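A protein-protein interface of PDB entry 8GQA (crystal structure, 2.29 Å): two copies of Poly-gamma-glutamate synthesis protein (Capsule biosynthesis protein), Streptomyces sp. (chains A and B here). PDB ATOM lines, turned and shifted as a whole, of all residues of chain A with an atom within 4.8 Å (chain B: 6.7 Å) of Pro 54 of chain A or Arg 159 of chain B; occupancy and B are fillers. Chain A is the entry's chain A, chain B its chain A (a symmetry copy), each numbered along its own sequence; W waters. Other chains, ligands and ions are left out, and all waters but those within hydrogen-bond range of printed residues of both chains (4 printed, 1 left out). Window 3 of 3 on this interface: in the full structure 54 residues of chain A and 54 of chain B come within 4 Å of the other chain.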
ATOM      1  N   GLY A  52      -9.365 -15.231 -12.617  1.00  0.00           N
ATOM      2  CA  GLY A  52     -10.255 -15.986 -11.758  1.00  0.00           C
ATOM      3  C   GLY A  52     -10.123 -15.588 -10.298  1.00  0.00           C
ATOM      4  O   GLY A  52      -9.403 -14.654  -9.931  1.00  0.00           O
ATOM      5  N   HIS A  53     -10.846 -16.328  -9.454  1.00  0.00           N
ATOM      6  CA  HIS A  53     -10.884 -16.095  -8.016  1.00  0.00           C
ATOM      7  C   HIS A  53     -10.894 -17.430  -7.284  1.00  0.00           C
ATOM      8  O   HIS A  53     -11.555 -18.378  -7.733  1.00  0.00           O
ATOM      9  CB  HIS A  53     -12.118 -15.278  -7.609  1.00  0.00           C
ATOM     10  CG  HIS A  53     -12.295 -14.019  -8.397  1.00  0.00           C
ATOM     11  ND1 HIS A  53     -11.662 -12.840  -8.067  1.00  0.00           N
ATOM     12  CD2 HIS A  53     -13.034 -13.752  -9.500  1.00  0.00           C
ATOM     13  CE1 HIS A  53     -12.003 -11.901  -8.932  1.00  0.00           C
ATOM     14  NE2 HIS A  53     -12.835 -12.429  -9.812  1.00  0.00           N
ATOM     15  N   PRO A  54     -10.193 -17.532  -6.156  1.00  0.00           N
ATOM     16  CA  PRO A  54     -10.110 -18.819  -5.456  1.00  0.00           C
ATOM     17  C   PRO A  54     -11.454 -19.233  -4.875  1.00  0.00           C
ATOM     18  O   PRO A  54     -12.175 -18.424  -4.286  1.00  0.00           O
ATOM     19  CB  PRO A  54      -9.081 -18.563  -4.345  1.00  0.00           C
ATOM     20  CG  PRO A  54      -8.461 -17.226  -4.659  1.00  0.00           C
ATOM     21  CD  PRO A  54      -9.478 -16.466  -5.436  1.00  0.00           C
ATOM     22  N   VAL A  55     -11.785 -20.508  -5.051  1.00  0.00           N
ATOM     23  CA  VAL A  55     -12.981 -21.087  -4.467  1.00  0.00           C
ATOM     24  C   VAL A  55     -12.595 -21.777  -3.166  1.00  0.00           C
ATOM     25  O   VAL A  55     -11.431 -22.110  -2.926  1.00  0.00           O
ATOM     26  CB  VAL A  55     -13.684 -22.072  -5.431  1.00  0.00           C
ATOM     27  CG1 VAL A  55     -13.838 -21.448  -6.809  1.00  0.00           C
ATOM     28  CG2 VAL A  55     -12.915 -23.382  -5.511  1.00  0.00           C
ATOM     29  N   HIS A  56     -13.587 -21.990  -2.305  1.00  0.00           N
ATOM     30  CA  HIS A  56     -13.358 -22.674  -1.036  1.00  0.00           C
ATOM     31  C   HIS A  56     -13.372 -24.176  -1.283  1.00  0.00           C
ATOM     32  O   HIS A  56     -14.428 -24.763  -1.539  1.00  0.00           O
ATOM     33  CB  HIS A  56     -14.406 -22.272  -0.004  1.00  0.00           C
ATOM     34  CG  HIS A  56     -14.079 -22.713   1.389  1.00  0.00           C
ATOM     35  ND1 HIS A  56     -14.978 -22.623   2.429  1.00  0.00           N
ATOM     36  CD2 HIS A  56     -12.950 -23.246   1.913  1.00  0.00           C
ATOM     37  CE1 HIS A  56     -14.417 -23.083   3.534  1.00  0.00           C
ATOM     38  NE2 HIS A  56     -13.186 -23.467   3.247  1.00  0.00           N
ATOM     39  N   CYS A  63      -6.473 -24.805  -2.119  1.00  0.00           N
ATOM     40  CA  CYS A  63      -6.287 -24.420  -3.508  1.00  0.00           C
ATOM     41  C   CYS A  63      -4.965 -24.960  -4.040  1.00  0.00           C
ATOM     42  O   CYS A  63      -3.970 -25.058  -3.315  1.00  0.00           O
ATOM     43  CB  CYS A  63      -6.327 -22.898  -3.650  1.00  0.00           C
ATOM     44  SG  CYS A  63      -7.996 -22.215  -3.787  1.00  0.00           S
ATOM     45  N   ASP A  91     -10.494 -24.622  -9.086  1.00  0.00           N
ATOM     46  CA  ASP A  91     -10.007 -23.904  -7.913  1.00  0.00           C
ATOM     47  C   ASP A  91     -10.022 -22.393  -8.104  1.00  0.00           C
ATOM     48  O   ASP A  91     -10.018 -21.657  -7.112  1.00  0.00           O
ATOM     49  CB  ASP A  91      -8.595 -24.371  -7.557  1.00  0.00           C
ATOM     50  CG  ASP A  91      -8.599 -25.604  -6.672  1.00  0.00           C
ATOM     51  OD1 ASP A  91      -9.699 -26.113  -6.369  1.00  0.00           O
ATOM     52  OD2 ASP A  91      -7.506 -26.061  -6.278  1.00  0.00           O
ATOM     53  N   LEU A  92     -10.031 -21.914  -9.348  1.00  0.00           N
ATOM     54  CA  LEU A  92     -10.164 -20.492  -9.636  1.00  0.00           C
ATOM     55  C   LEU A  92     -11.507 -20.160 -10.279  1.00  0.00           C
ATOM     56  O   LEU A  92     -11.654 -19.096 -10.889  1.00  0.00           O
ATOM     57  CB  LEU A  92      -9.011 -20.014 -10.519  1.00  0.00           C
ATOM     58  CG  LEU A  92      -7.691 -19.750  -9.792  1.00  0.00           C
ATOM     59  CD1 LEU A  92      -6.582 -19.414 -10.779  1.00  0.00           C
ATOM     60  CD2 LEU A  92      -7.856 -18.635  -8.766  1.00  0.00           C
ATOM     61  N   SER A 326      -4.766 -19.346  -0.465  1.00  0.00           N
ATOM     62  CA  SER A 326      -5.902 -18.450  -0.321  1.00  0.00           C
ATOM     63  C   SER A 326      -6.156 -18.122   1.148  1.00  0.00           C
ATOM     64  O   SER A 326      -5.665 -18.794   2.060  1.00  0.00           O
ATOM     65  CB  SER A 326      -7.155 -19.064  -0.946  1.00  0.00           C
ATOM     66  OG  SER A 326      -7.796 -19.950  -0.046  1.00  0.00           O
ATOM     67  N   GLU A 328      -8.981 -18.294   2.871  1.00  0.00           N
ATOM     68  CA  GLU A 328      -9.728 -19.351   3.543  1.00  0.00           C
ATOM     69  C   GLU A 328      -8.832 -20.535   3.887  1.00  0.00           C
ATOM     70  O   GLU A 328      -9.029 -21.178   4.924  1.00  0.00           O
ATOM     71  CB  GLU A 328     -10.901 -19.801   2.675  1.00  0.00           C
ATOM     72  CG  GLU A 328     -12.025 -18.780   2.580  1.00  0.00           C
ATOM     73  CD  GLU A 328     -12.930 -19.014   1.387  1.00  0.00           C
ATOM     74  OE1 GLU A 328     -12.411 -19.348   0.301  1.00  0.00           O
ATOM     75  OE2 GLU A 328     -14.161 -18.861   1.534  1.00  0.00           O
ATOM     76  N   MET B  90     -26.162 -14.769  -6.519  1.00  0.00           N
ATOM     77  CA  MET B  90     -25.080 -15.489  -7.173  1.00  0.00           C
ATOM     78  C   MET B  90     -25.577 -16.411  -8.281  1.00  0.00           C
ATOM     79  O   MET B  90     -24.863 -17.341  -8.671  1.00  0.00           O
ATOM     80  CB  MET B  90     -24.283 -16.291  -6.143  1.00  0.00           C
ATOM     81  CG  MET B  90     -23.598 -15.436  -5.094  1.00  0.00           C
ATOM     82  SD  MET B  90     -22.392 -14.317  -5.827  1.00  0.00           S
ATOM     83  CE  MET B  90     -21.181 -15.491  -6.428  1.00  0.00           C
ATOM     84  N   THR B  94     -19.747 -15.505  -9.907  1.00  0.00           N
ATOM     85  CA  THR B  94     -18.934 -14.365  -9.496  1.00  0.00           C
ATOM     86  C   THR B  94     -18.957 -13.263 -10.547  1.00  0.00           C
ATOM     87  O   THR B  94     -18.969 -12.073 -10.212  1.00  0.00           O
ATOM     88  CB  THR B  94     -17.498 -14.814  -9.229  1.00  0.00           C
ATOM     89  OG1 THR B  94     -16.959 -15.423 -10.410  1.00  0.00           O
ATOM     90  CG2 THR B  94     -17.459 -15.816  -8.085  1.00  0.00           C
ATOM     91  N   GLY B 115     -20.182  -7.859  -2.744  1.00  0.00           N
ATOM     92  CA  GLY B 115     -18.968  -7.110  -3.015  1.00  0.00           C
ATOM     93  C   GLY B 115     -17.966  -7.953  -3.768  1.00  0.00           C
ATOM     94  O   GLY B 115     -18.165  -9.151  -3.989  1.00  0.00           O
ATOM     95  N   ALA B 116     -16.872  -7.297  -4.166  1.00  0.00           N
ATOM     96  CA  ALA B 116     -15.783  -7.998  -4.834  1.00  0.00           C
ATOM     97  C   ALA B 116     -14.988  -8.871  -3.873  1.00  0.00           C
ATOM     98  O   ALA B 116     -14.246  -9.750  -4.323  1.00  0.00           O
ATOM     99  CB  ALA B 116     -14.856  -6.999  -5.528  1.00  0.00           C
ATOM    100  N   ASP B 117     -15.119  -8.644  -2.568  1.00  0.00           N
ATOM    101  CA  ASP B 117     -14.539  -9.521  -1.562  1.00  0.00           C
ATOM    102  C   ASP B 117     -15.443  -9.505  -0.334  1.00  0.00           C
ATOM    103  O   ASP B 117     -16.492  -8.854  -0.319  1.00  0.00           O
ATOM    104  CB  ASP B 117     -13.093  -9.123  -1.231  1.00  0.00           C
ATOM    105  CG  ASP B 117     -12.953  -7.662  -0.839  1.00  0.00           C
ATOM    106  OD1 ASP B 117     -13.956  -7.036  -0.436  1.00  0.00           O
ATOM    107  OD2 ASP B 117     -11.822  -7.137  -0.931  1.00  0.00           O
ATOM    108  N   LEU B 118     -15.022 -10.228   0.708  1.00  0.00           N
ATOM    109  CA  LEU B 118     -15.872 -10.396   1.884  1.00  0.00           C
ATOM    110  C   LEU B 118     -16.081  -9.078   2.618  1.00  0.00           C
ATOM    111  O   LEU B 118     -17.204  -8.765   3.032  1.00  0.00           O
ATOM    112  CB  LEU B 118     -15.274 -11.441   2.823  1.00  0.00           C
ATOM    113  CG  LEU B 118     -16.059 -11.704   4.111  1.00  0.00           C
ATOM    114  CD1 LEU B 118     -17.521 -12.005   3.806  1.00  0.00           C
ATOM    115  CD2 LEU B 118     -15.428 -12.843   4.897  1.00  0.00           C
ATOM    116  N   GLY B 146     -20.082 -21.999  -0.453  1.00  0.00           N
ATOM    117  CA  GLY B 146     -19.120 -21.481  -1.394  1.00  0.00           C
ATOM    118  C   GLY B 146     -19.500 -20.158  -2.024  1.00  0.00           C
ATOM    119  O   GLY B 146     -18.628 -19.477  -2.576  1.00  0.00           O
ATOM    120  N   GLN B 147     -20.777 -19.771  -1.954  1.00  0.00           N
ATOM    121  CA  GLN B 147     -21.219 -18.512  -2.543  1.00  0.00           C
ATOM    122  C   GLN B 147     -20.855 -17.304  -1.695  1.00  0.00           C
ATOM    123  O   GLN B 147     -20.925 -16.174  -2.193  1.00  0.00           O
ATOM    124  CB  GLN B 147     -22.732 -18.532  -2.767  1.00  0.00           C
ATOM    125  CG  GLN B 147     -23.173 -19.393  -3.935  1.00  0.00           C
ATOM    126  CD  GLN B 147     -24.656 -19.267  -4.218  1.00  0.00           C
ATOM    127  OE1 GLN B 147     -25.423 -18.803  -3.374  1.00  0.00           O
ATOM    128  NE2 GLN B 147     -25.067 -19.679  -5.411  1.00  0.00           N
ATOM    129  N   GLU B 148     -20.485 -17.508  -0.433  1.00  0.00           N
ATOM    130  CA  GLU B 148     -20.040 -16.396   0.392  1.00  0.00           C
ATOM    131  C   GLU B 148     -18.786 -15.774  -0.209  1.00  0.00           C
ATOM    132  O   GLU B 148     -17.950 -16.465  -0.797  1.00  0.00           O
ATOM    133  CB  GLU B 148     -19.771 -16.864   1.824  1.00  0.00           C
ATOM    134  CG  GLU B 148     -18.499 -17.689   2.003  1.00  0.00           C
ATOM    135  CD  GLU B 148     -18.709 -19.162   1.705  1.00  0.00           C
ATOM    136  OE1 GLU B 148     -19.829 -19.536   1.299  1.00  0.00           O
ATOM    137  OE2 GLU B 148     -17.753 -19.947   1.880  1.00  0.00           O
ATOM    138  N   ALA B 149     -18.673 -14.458  -0.082  1.00  0.00           N
ATOM    139  CA  ALA B 149     -17.482 -13.782  -0.566  1.00  0.00           C
ATOM    140  C   ALA B 149     -16.279 -14.165   0.288  1.00  0.00           C
ATOM    141  O   ALA B 149     -16.407 -14.678   1.403  1.00  0.00           O
ATOM    142  CB  ALA B 149     -17.683 -12.267  -0.559  1.00  0.00           C
ATOM    143  N   ALA B 150     -15.092 -13.916  -0.254  1.00  0.00           N
ATOM    144  CA  ALA B 150     -13.848 -14.207   0.440  1.00  0.00           C
ATOM    145  C   ALA B 150     -12.937 -12.992   0.374  1.00  0.00           C
ATOM    146  O   ALA B 150     -12.923 -12.260  -0.618  1.00  0.00           O
ATOM    147  CB  ALA B 150     -13.138 -15.432  -0.155  1.00  0.00           C
ATOM    148  N   ASP B 151     -12.188 -12.780   1.444  1.00  0.00           N
ATOM    149  CA  ASP B 151     -11.221 -11.698   1.506  1.00  0.00           C
ATOM    150  C   ASP B 151      -9.900 -12.137   0.889  1.00  0.00           C
ATOM    151  O   ASP B 151      -9.628 -13.335   0.763  1.00  0.00           O
ATOM    152  CB  ASP B 151     -11.018 -11.266   2.956  1.00  0.00           C
ATOM    153  CG  ASP B 151     -11.898 -10.092   3.337  1.00  0.00           C
ATOM    154  OD1 ASP B 151     -12.375  -9.387   2.422  1.00  0.00           O
ATOM    155  OD2 ASP B 151     -12.113  -9.874   4.548  1.00  0.00           O
ATOM    156  N   PRO B 152      -9.057 -11.196   0.473  1.00  0.00           N
ATOM    157  CA  PRO B 152      -7.788 -11.574  -0.153  1.00  0.00           C
ATOM    158  C   PRO B 152      -6.766 -12.053   0.866  1.00  0.00           C
ATOM    159  O   PRO B 152      -6.837 -11.758   2.061  1.00  0.00           O
ATOM    160  CB  PRO B 152      -7.314 -10.279  -0.833  1.00  0.00           C
ATOM    161  CG  PRO B 152      -8.449  -9.298  -0.698  1.00  0.00           C
ATOM    162  CD  PRO B 152      -9.246  -9.736   0.480  1.00  0.00           C
ATOM    163  N   LEU B 156      -3.231 -14.275  -3.125  1.00  0.00           N
ATOM    164  CA  LEU B 156      -4.366 -14.471  -4.008  1.00  0.00           C
ATOM    165  C   LEU B 156      -5.426 -13.417  -3.738  1.00  0.00           C
ATOM    166  O   LEU B 156      -5.558 -12.936  -2.607  1.00  0.00           O
ATOM    167  CB  LEU B 156      -4.975 -15.869  -3.827  1.00  0.00           C
ATOM    168  CG  LEU B 156      -4.122 -17.042  -4.317  1.00  0.00           C
ATOM    169  CD1 LEU B 156      -4.735 -18.368  -3.897  1.00  0.00           C
ATOM    170  CD2 LEU B 156      -3.944 -16.982  -5.826  1.00  0.00           C
ATOM    171  N   PRO B 157      -6.192 -13.035  -4.755  1.00  0.00           N
ATOM    172  CA  PRO B 157      -7.301 -12.105  -4.532  1.00  0.00           C
ATOM    173  C   PRO B 157      -8.404 -12.762  -3.718  1.00  0.00           C
ATOM    174  O   PRO B 157      -8.386 -13.959  -3.424  1.00  0.00           O
ATOM    175  CB  PRO B 157      -7.780 -11.773  -5.947  1.00  0.00           C
ATOM    176  CG  PRO B 157      -7.383 -12.962  -6.758  1.00  0.00           C
ATOM    177  CD  PRO B 157      -6.079 -13.428  -6.172  1.00  0.00           C
ATOM    178  N   GLY B 158      -9.382 -11.947  -3.354  1.00  0.00           N
ATOM    179  CA  GLY B 158     -10.586 -12.444  -2.727  1.00  0.00           C
ATOM    180  C   GLY B 158     -11.482 -13.125  -3.740  1.00  0.00           C
ATOM    181  O   GLY B 158     -11.072 -13.465  -4.853  1.00  0.00           O
ATOM    182  N   ARG B 159     -12.734 -13.328  -3.340  1.00  0.00           N
ATOM    183  CA  ARG B 159     -13.737 -13.890  -4.223  1.00  0.00           C
ATOM    184  C   ARG B 159     -15.009 -13.058  -4.093  1.00  0.00           C
ATOM    185  O   ARG B 159     -15.493 -12.838  -2.969  1.00  0.00           O
ATOM    186  CB  ARG B 159     -14.022 -15.363  -3.895  1.00  0.00           C
ATOM    187  CG  ARG B 159     -15.125 -15.971  -4.748  1.00  0.00           C
ATOM    188  CD  ARG B 159     -15.368 -17.430  -4.402  1.00  0.00           C
ATOM    189  NE  ARG B 159     -15.889 -17.596  -3.050  1.00  0.00           N
ATOM    190  CZ  ARG B 159     -15.194 -18.104  -2.038  1.00  0.00           C
ATOM    191  NH1 ARG B 159     -13.942 -18.499  -2.223  1.00  0.00           N
ATOM    192  NH2 ARG B 159     -15.752 -18.217  -0.840  1.00  0.00           N
ATOM    193  N   PRO B 160     -15.559 -12.563  -5.199  1.00  0.00           N
ATOM    194  CA  PRO B 160     -16.844 -11.860  -5.125  1.00  0.00           C
ATOM    195  C   PRO B 160     -17.934 -12.791  -4.619  1.00  0.00           C
ATOM    196  O   PRO B 160     -17.933 -13.993  -4.899  1.00  0.00           O
ATOM    197  CB  PRO B 160     -17.102 -11.429  -6.574  1.00  0.00           C
ATOM    198  CG  PRO B 160     -15.761 -11.490  -7.244  1.00  0.00           C
ATOM    199  CD  PRO B 160     -15.018 -12.596  -6.567  1.00  0.00           C
ATOM    200  N   GLY B 161     -18.865 -12.228  -3.857  1.00  0.00           N
ATOM    201  CA  GLY B 161     -19.935 -13.031  -3.298  1.00  0.00           C
ATOM    202  C   GLY B 161     -20.786 -12.226  -2.336  1.00  0.00           C
ATOM    203  O   GLY B 161     -20.778 -10.993  -2.356  1.00  0.00           O
ATOM    204  N   LEU B 162     -21.512 -12.951  -1.491  1.00  0.00           N
ATOM    205  CA  LEU B 162     -22.497 -12.377  -0.589  1.00  0.00           C
ATOM    206  C   LEU B 162     -21.963 -12.307   0.838  1.00  0.00           C
ATOM    207  O   LEU B 162     -20.947 -12.913   1.187  1.00  0.00           O
ATOM    208  CB  LEU B 162     -23.795 -13.191  -0.637  1.00  0.00           C
ATOM    209  CG  LEU B 162     -23.667 -14.720  -0.622  1.00  0.00           C
ATOM    210  CD1 LEU B 162     -23.545 -15.266   0.796  1.00  0.00           C
ATOM    211  CD2 LEU B 162     -24.841 -15.364  -1.346  1.00  0.00           C
HETATM  212  O   HOH W   1     -14.405 -17.371 -11.513  1.00  0.00           O
HETATM  213  O   HOH W   2     -14.926 -16.299   3.149  1.00  0.00           O
HETATM  214  O   HOH W   3     -17.752 -23.111   1.880  1.00  0.00           O
HETATM  215  O   HOH W   4     -16.270 -20.932  -3.255  1.00  0.00           O
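Of the printed residues of chain B, His 53 of chain A touches Gly 158 and Pro 160. Pro 54 of chain A touches just these residues of chain B: Leu 156 (3.8 Å), Pro 157 (3.4 Å), Gly 158 (3.4 Å) and Arg 159 (2.7 Å). Of the printed residues of chain B, Val 55 of chain A touches Arg 159 (3.6 Å). Of the printed residues of chain B, Ser 326 of chain A touches Leu 156 (3.6 Å). Of the printed residues of chain A, Glu 148 of chain B touches His 56 (3.9 Å) and Glu 328 (3.8 Å). Asp 151 of chain B touches none of the printed residues of chain A. Of the printed residues of chain A, Leu 156 of chain B touches Pro 54 and Ser 326. The nearest residue of chain B that does not touch Pro 54 of chain A is Ala 150 of chain B (5.2 Å). The nearest printed residue of chain A that does not touch Pro 157 of chain B is Gly 52 of chain A (4.1 Å).
Printed residues of chain A that touch a printed residue of chain B: His 53, Pro 54, Val 55, His 56, Ser 326 and Glu 328. Hydrophobic or aromatic side chains of chain A that line the printed part of chain B: His 53, Pro 54 and His 56. Along chain A the printed residues that touch a printed residue of chain B span positions 53 to 328. Of the 20 printed residues of chain B, 7 touch a printed residue of chain A. Printed residues of chain B that touch a printed residue of chain A: Glu 148, Ala 150, Leu 156, Pro 157, Gly 158, Arg 159 and Pro 160. Hydrophobic or aromatic side chains of chain B within 4 Å of the printed part of chain A: Ala 150, Leu 156 and Pro 160. Among the printed residues, Asp or Glu carboxylates within 4 Å of a Lys or Arg side-chain nitrogen of the other chain: Glu 328 of chain A with Arg 159 of chain B (2.9 Å).
Water W2 bridges O of Ala 149 of chain B (2.8 Å) and OE2 of Glu 328 of chain A (3.1 Å). Water W4 lies within hydrogen-bond range of the backbone carbonyl oxygen (O) of Gly 146 of chain B (2.9 Å), the backbone NH (N) of His 56 of chain A (3.0 Å) and the guanidinium group (NE) of Arg 159 of chain B (3.4 Å). Water W3 lies within hydrogen-bond range of ND1 of His 56 of chain A (2.9 Å), OE2 of Glu 148 of chain B (3.2 Å) and N of Gly 146 of chain B (3.5 Å). Water W1 bridges the backbone carbonyl oxygen of Leu 92 of chain A and the side-chain hydroxyl of Thr 94 of chain B.
No position is printed for both chains.
Pro 160 of chain B touches His 53 of chain A. CB of Leu 156 of chain B touches CG of Pro 54 of chain A, 3.8 Å away. Pro 54 of chain A touches Pro 157 of chain B (CD to O, 3.4 Å). O of Gly 158 of chain B touches CD of Pro 54 of chain A, 3.4 Å away. Val 55 of chain A touches Arg 159 of chain B (CA to NH1, 3.6 Å). His 56 of chain A touches Glu 148 of chain B. His 56 of chain A touches Arg 159 of chain B. CD1 of Leu 156 of chain B touches N of Ser 326 of chain A, 3.6 Å away. OE2 of Glu 148 of chain B touches OE2 of Glu 328 of chain A (3.8 Å). Glu 328 of chain A touches Ala 150 of chain B.
NH2 of Arg 159 of chain B is in salt-bridge range of OE2 of Glu 328 of chain A. NH1 of Arg 159 of chain B lies within hydrogen-bond range of O of Pro 54 of chain A (2.7 Å). O of Gly 158 of chain B sits at hydrogen-bond distance from ND1 of His 53 of chain A (3.3 Å).
O of Gly 146 of chain B lies within hydrogen-bond range of NE of Arg 159 of chain B (3.4 Å). The side-chain sulfur (SG) of Cys 63 of chain A sits at hydrogen-bond distance from the backbone carbonyl oxygen (O) of Val 55 of chain A, 3.5 Å away. The backbone NH (N) of His 53 of chain A is in hydrogen-bond range of the backbone carbonyl oxygen (O) of Leu 92 of chain A (3.2 Å). The side-chain carboxylate of Glu 148 of chain B lies within salt-bridge range of the guanidinium group of Arg 159 of chain B (3.8 Å). N of Val 55 of chain A lies within hydrogen-bond range of O of Asp 91 of chain A. The backbone NH of Arg 159 of chain B sits at hydrogen-bond distance from the backbone carbonyl oxygen of Ala 150 of chain B.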
